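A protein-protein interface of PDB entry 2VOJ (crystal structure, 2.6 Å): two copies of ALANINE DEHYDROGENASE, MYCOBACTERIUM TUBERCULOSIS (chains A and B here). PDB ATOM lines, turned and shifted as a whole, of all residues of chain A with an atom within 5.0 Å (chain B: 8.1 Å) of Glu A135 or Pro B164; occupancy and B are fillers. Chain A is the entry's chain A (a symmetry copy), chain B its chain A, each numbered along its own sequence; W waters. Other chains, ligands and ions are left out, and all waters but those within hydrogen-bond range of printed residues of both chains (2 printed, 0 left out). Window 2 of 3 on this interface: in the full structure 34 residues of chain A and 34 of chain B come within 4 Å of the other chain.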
ATOM      1  N   ALA A 131      29.188  12.717 -34.933  1.00  0.00           N
ATOM      2  CA  ALA A 131      28.720  12.800 -33.541  1.00  0.00           C
ATOM      3  C   ALA A 131      28.639  11.445 -32.809  1.00  0.00           C
ATOM      4  O   ALA A 131      29.237  11.308 -31.775  1.00  0.00           O
ATOM      5  CB  ALA A 131      27.391  13.624 -33.401  1.00  0.00           C
ATOM      6  N   PRO A 132      27.926  10.441 -33.365  1.00  0.00           N
ATOM      7  CA  PRO A 132      27.870   9.161 -32.631  1.00  0.00           C
ATOM      8  C   PRO A 132      29.221   8.469 -32.453  1.00  0.00           C
ATOM      9  O   PRO A 132      29.421   7.792 -31.452  1.00  0.00           O
ATOM     10  CB  PRO A 132      26.884   8.304 -33.437  1.00  0.00           C
ATOM     11  CG  PRO A 132      26.706   9.003 -34.743  1.00  0.00           C
ATOM     12  CD  PRO A 132      27.143  10.415 -34.622  1.00  0.00           C
ATOM     13  N   MET A 133      30.154   8.653 -33.374  1.00  0.00           N
ATOM     14  CA  MET A 133      31.485   8.125 -33.148  1.00  0.00           C
ATOM     15  C   MET A 133      32.304   8.965 -32.137  1.00  0.00           C
ATOM     16  O   MET A 133      33.188   8.427 -31.471  1.00  0.00           O
ATOM     17  CB  MET A 133      32.210   7.903 -34.487  1.00  0.00           C
ATOM     18  CG  MET A 133      31.451   6.971 -35.434  1.00  0.00           C
ATOM     19  SD  MET A 133      31.223   5.328 -34.709  1.00  0.00           S
ATOM     20  CE  MET A 133      29.585   5.348 -33.978  1.00  0.00           C
ATOM     21  N   SER A 134      32.015  10.263 -32.015  1.00  0.00           N
ATOM     22  CA  SER A 134      32.662  11.075 -30.986  1.00  0.00           C
ATOM     23  C   SER A 134      32.121  10.735 -29.599  1.00  0.00           C
ATOM     24  O   SER A 134      32.852  10.757 -28.615  1.00  0.00           O
ATOM     25  CB  SER A 134      32.512  12.564 -31.226  1.00  0.00           C
ATOM     26  OG  SER A 134      33.171  12.913 -32.407  1.00  0.00           O
ATOM     27  N   GLU A 135      30.844  10.398 -29.517  1.00  0.00           N
ATOM     28  CA  GLU A 135      30.290   9.907 -28.252  1.00  0.00           C
ATOM     29  C   GLU A 135      30.975   8.615 -27.794  1.00  0.00           C
ATOM     30  O   GLU A 135      31.358   8.511 -26.650  1.00  0.00           O
ATOM     31  CB  GLU A 135      28.761   9.706 -28.353  1.00  0.00           C
ATOM     32  CG  GLU A 135      28.008  10.954 -28.848  1.00  0.00           C
ATOM     33  CD  GLU A 135      26.540  10.741 -29.056  1.00  0.00           C
ATOM     34  OE1 GLU A 135      26.173   9.767 -29.752  1.00  0.00           O
ATOM     35  OE2 GLU A 135      25.740  11.563 -28.537  1.00  0.00           O
ATOM     36  N   VAL A 136      31.105   7.634 -28.684  1.00  0.00           N
ATOM     37  CA  VAL A 136      31.773   6.396 -28.352  1.00  0.00           C
ATOM     38  C   VAL A 136      33.233   6.648 -27.965  1.00  0.00           C
ATOM     39  O   VAL A 136      33.687   6.143 -26.940  1.00  0.00           O
ATOM     40  CB  VAL A 136      31.667   5.361 -29.522  1.00  0.00           C
ATOM     41  CG1 VAL A 136      32.482   4.106 -29.219  1.00  0.00           C
ATOM     42  CG2 VAL A 136      30.182   5.010 -29.806  1.00  0.00           C
ATOM     43  N   ALA A 137      33.947   7.451 -28.765  1.00  0.00           N
ATOM     44  CA  ALA A 137      35.373   7.640 -28.561  1.00  0.00           C
ATOM     45  C   ALA A 137      35.642   8.468 -27.294  1.00  0.00           C
ATOM     46  O   ALA A 137      36.605   8.209 -26.565  1.00  0.00           O
ATOM     47  CB  ALA A 137      36.024   8.261 -29.782  1.00  0.00           C
ATOM     48  N   GLY A 138      34.775   9.439 -27.029  1.00  0.00           N
ATOM     49  CA  GLY A 138      34.903  10.266 -25.847  1.00  0.00           C
ATOM     50  C   GLY A 138      34.743   9.404 -24.609  1.00  0.00           C
ATOM     51  O   GLY A 138      35.552   9.478 -23.697  1.00  0.00           O
ATOM     52  N   ARG A 139      33.714   8.563 -24.585  1.00  0.00           N
ATOM     53  CA  ARG A 139      33.523   7.623 -23.469  1.00  0.00           C
ATOM     54  C   ARG A 139      34.644   6.589 -23.377  1.00  0.00           C
ATOM     55  O   ARG A 139      35.146   6.325 -22.287  1.00  0.00           O
ATOM     56  CB  ARG A 139      32.131   6.970 -23.522  1.00  0.00           C
ATOM     57  CG  ARG A 139      31.004   8.021 -23.465  1.00  0.00           C
ATOM     58  CD  ARG A 139      29.602   7.473 -23.463  1.00  0.00           C
ATOM     59  NE  ARG A 139      28.664   8.589 -23.532  1.00  0.00           N
ATOM     60  CZ  ARG A 139      27.369   8.538 -23.217  1.00  0.00           C
ATOM     61  NH1 ARG A 139      26.802   7.414 -22.809  1.00  0.00           N
ATOM     62  NH2 ARG A 139      26.640   9.635 -23.295  1.00  0.00           N
ATOM     63  N   LEU A 140      35.083   6.045 -24.514  1.00  0.00           N
ATOM     64  CA  LEU A 140      36.249   5.172 -24.513  1.00  0.00           C
ATOM     65  C   LEU A 140      37.503   5.832 -23.959  1.00  0.00           C
ATOM     66  O   LEU A 140      38.234   5.203 -23.212  1.00  0.00           O
ATOM     67  CB  LEU A 140      36.541   4.587 -25.893  1.00  0.00           C
ATOM     68  CG  LEU A 140      35.685   3.358 -26.246  1.00  0.00           C
ATOM     69  CD1 LEU A 140      35.933   2.937 -27.689  1.00  0.00           C
ATOM     70  CD2 LEU A 140      35.934   2.199 -25.280  1.00  0.00           C
ATOM     71  N   THR A 178      31.524  17.354 -28.865  1.00  0.00           N
ATOM     72  CA  THR A 178      30.911  16.041 -28.567  1.00  0.00           C
ATOM     73  C   THR A 178      31.826  15.029 -27.850  1.00  0.00           C
ATOM     74  O   THR A 178      31.415  14.430 -26.823  1.00  0.00           O
ATOM     75  CB  THR A 178      30.337  15.384 -29.841  1.00  0.00           C
ATOM     76  OG1 THR A 178      29.415  16.279 -30.445  1.00  0.00           O
ATOM     77  CG2 THR A 178      29.631  14.042 -29.548  1.00  0.00           C
ATOM     78  N   ALA A 179      33.029  14.813 -28.383  1.00  0.00           N
ATOM     79  CA  ALA A 179      33.953  13.859 -27.785  1.00  0.00           C
ATOM     80  C   ALA A 179      34.460  14.394 -26.428  1.00  0.00           C
ATOM     81  O   ALA A 179      34.490  13.646 -25.461  1.00  0.00           O
ATOM     82  CB  ALA A 179      35.134  13.542 -28.731  1.00  0.00           C
ATOM     83  N   ASN A 182      31.801  14.174 -23.725  1.00  0.00           N
ATOM     84  CA  ASN A 182      31.637  12.777 -23.343  1.00  0.00           C
ATOM     85  C   ASN A 182      32.802  12.182 -22.528  1.00  0.00           C
ATOM     86  O   ASN A 182      32.575  11.415 -21.609  1.00  0.00           O
ATOM     87  CB  ASN A 182      31.274  11.908 -24.558  1.00  0.00           C
ATOM     88  CG  ASN A 182      29.795  11.963 -24.880  1.00  0.00           C
ATOM     89  OD1 ASN A 182      29.358  12.710 -25.764  1.00  0.00           O
ATOM     90  ND2 ASN A 182      29.010  11.216 -24.131  1.00  0.00           N
ATOM     91  N   LEU B 159      29.999  -0.786 -24.944  1.00  0.00           N
ATOM     92  CA  LEU B 159      30.476   0.323 -24.134  1.00  0.00           C
ATOM     93  C   LEU B 159      29.676   0.375 -22.822  1.00  0.00           C
ATOM     94  O   LEU B 159      28.449   0.299 -22.854  1.00  0.00           O
ATOM     95  CB  LEU B 159      30.298   1.598 -24.934  1.00  0.00           C
ATOM     96  CG  LEU B 159      30.763   2.932 -24.396  1.00  0.00           C
ATOM     97  CD1 LEU B 159      32.235   2.908 -24.076  1.00  0.00           C
ATOM     98  CD2 LEU B 159      30.466   3.916 -25.480  1.00  0.00           C
ATOM     99  N   GLY B 161      28.542   2.634 -20.845  1.00  0.00           N
ATOM    100  CA  GLY B 161      27.478   3.622 -20.732  1.00  0.00           C
ATOM    101  C   GLY B 161      26.583   3.753 -21.935  1.00  0.00           C
ATOM    102  O   GLY B 161      25.644   4.549 -21.932  1.00  0.00           O
ATOM    103  N   GLY B 162      26.831   2.946 -22.960  1.00  0.00           N
ATOM    104  CA  GLY B 162      26.168   3.112 -24.248  1.00  0.00           C
ATOM    105  C   GLY B 162      26.373   4.526 -24.779  1.00  0.00           C
ATOM    106  O   GLY B 162      27.293   5.252 -24.339  1.00  0.00           O
ATOM    107  N   VAL B 163      25.531   4.918 -25.732  1.00  0.00           N
ATOM    108  CA  VAL B 163      25.442   6.292 -26.220  1.00  0.00           C
ATOM    109  C   VAL B 163      23.957   6.575 -26.439  1.00  0.00           C
ATOM    110  O   VAL B 163      23.192   5.647 -26.499  1.00  0.00           O
ATOM    111  CB  VAL B 163      26.269   6.535 -27.550  1.00  0.00           C
ATOM    112  CG1 VAL B 163      27.748   6.480 -27.297  1.00  0.00           C
ATOM    113  CG2 VAL B 163      25.858   5.561 -28.679  1.00  0.00           C
ATOM    114  N   PRO B 164      23.557   7.856 -26.567  1.00  0.00           N
ATOM    115  CA  PRO B 164      22.125   8.110 -26.717  1.00  0.00           C
ATOM    116  C   PRO B 164      21.539   7.242 -27.837  1.00  0.00           C
ATOM    117  O   PRO B 164      22.089   7.200 -28.929  1.00  0.00           O
ATOM    118  CB  PRO B 164      22.070   9.592 -27.085  1.00  0.00           C
ATOM    119  CG  PRO B 164      23.372  10.166 -26.490  1.00  0.00           C
ATOM    120  CD  PRO B 164      24.374   9.092 -26.614  1.00  0.00           C
ATOM    121  N   GLY B 165      20.445   6.531 -27.548  1.00  0.00           N
ATOM    122  CA  GLY B 165      19.755   5.733 -28.543  1.00  0.00           C
ATOM    123  C   GLY B 165      20.160   4.263 -28.546  1.00  0.00           C
ATOM    124  O   GLY B 165      19.496   3.419 -29.177  1.00  0.00           O
ATOM    125  N   VAL B 166      21.234   3.938 -27.829  1.00  0.00           N
ATOM    126  CA  VAL B 166      21.720   2.583 -27.757  1.00  0.00           C
ATOM    127  C   VAL B 166      21.887   2.168 -26.277  1.00  0.00           C
ATOM    128  O   VAL B 166      22.405   2.940 -25.469  1.00  0.00           O
ATOM    129  CB  VAL B 166      23.105   2.451 -28.503  1.00  0.00           C
ATOM    130  CG1 VAL B 166      23.673   1.039 -28.389  1.00  0.00           C
ATOM    131  CG2 VAL B 166      23.008   2.866 -29.959  1.00  0.00           C
ATOM    132  N   GLU B 167      21.501   0.936 -25.938  1.00  0.00           N
ATOM    133  CA  GLU B 167      21.514   0.483 -24.543  1.00  0.00           C
ATOM    134  C   GLU B 167      22.913   0.392 -23.880  1.00  0.00           C
ATOM    135  O   GLU B 167      23.902  -0.006 -24.514  1.00  0.00           O
ATOM    136  CB  GLU B 167      20.777  -0.865 -24.406  1.00  0.00           C
ATOM    137  CG  GLU B 167      21.515  -2.065 -25.039  1.00  0.00           C
ATOM    138  CD  GLU B 167      20.947  -3.444 -24.610  1.00  0.00           C
ATOM    139  OE1 GLU B 167      20.051  -3.486 -23.710  1.00  0.00           O
ATOM    140  OE2 GLU B 167      21.419  -4.491 -25.158  1.00  0.00           O
HETATM  141  O   HOH W   1      24.316   8.362 -30.718  1.00  0.00           O
HETATM  142  O   HOH W   2      23.901   7.277 -22.925  1.00  0.00           O
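NH1 of Arg A139 is in hydrogen-bond range of O of Gly B161, 3.2 Å away.
The guanidinium group (NH1) of Arg A139 lies within hydrogen-bond range of the backbone carbonyl oxygen (O) of Gly B162 (2.7 Å).
ND2 of Asn A182 sits close to NE of Arg A139.
CG1 of Val B163 touches CB of Glu A135 (3.5 Å).
Pro B164 touches Glu A135.
CG2 of Val A136 touches CG1 of Val B163, 3.8 Å away.
Arg A139 touches Leu B159.
NH1 of Arg A139 touches CA of Val B163, at 3.8 Å.
Leu A140 touches Leu B159.
Glu A135 touches just these residues of chain B: Val B163 and Pro B164.
Pro B164 touches one residue of chain A.
Printed residues of chain A within 4 Å of Val B163: Glu A135, Val A136 and Arg A139.
Of the printed residues of chain A, Gly B161 touches Arg A139.
Printed residues of chain B within 4 Å of Leu A140: Leu B159.
The nearest residue of chain B that does not touch Glu A135 is Leu B159 (4.8 Å).
Of the 13 printed residues of chain A, 4 touch a printed residue of chain B.
Printed residues of chain A that touch a printed residue of chain B: Glu A135, Val A136, Arg A139 and Leu A140.
Hydrophobic or aromatic side chains of chain A within 4 Å of the printed part of chain B: Val A136 and Leu A140.
Hydrophobic or aromatic side chains of chain B that line the printed part of chain A: Leu B159, Val B163 and Pro B164.
Among the printed residues, 8 pairs touch across the chains.
No position is printed for both chains.
Water W1 bridges the side-chain carboxylate (OE1) of Glu A135 (2.5 Å) and the backbone carbonyl oxygen (O) of Pro B164 (3.1 Å).
Water W2 lies within hydrogen-bond range of the guanidinium group of Arg A139 (2.9 Å) and the backbone carbonyl oxygen of Gly B161 (3.4 Å).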
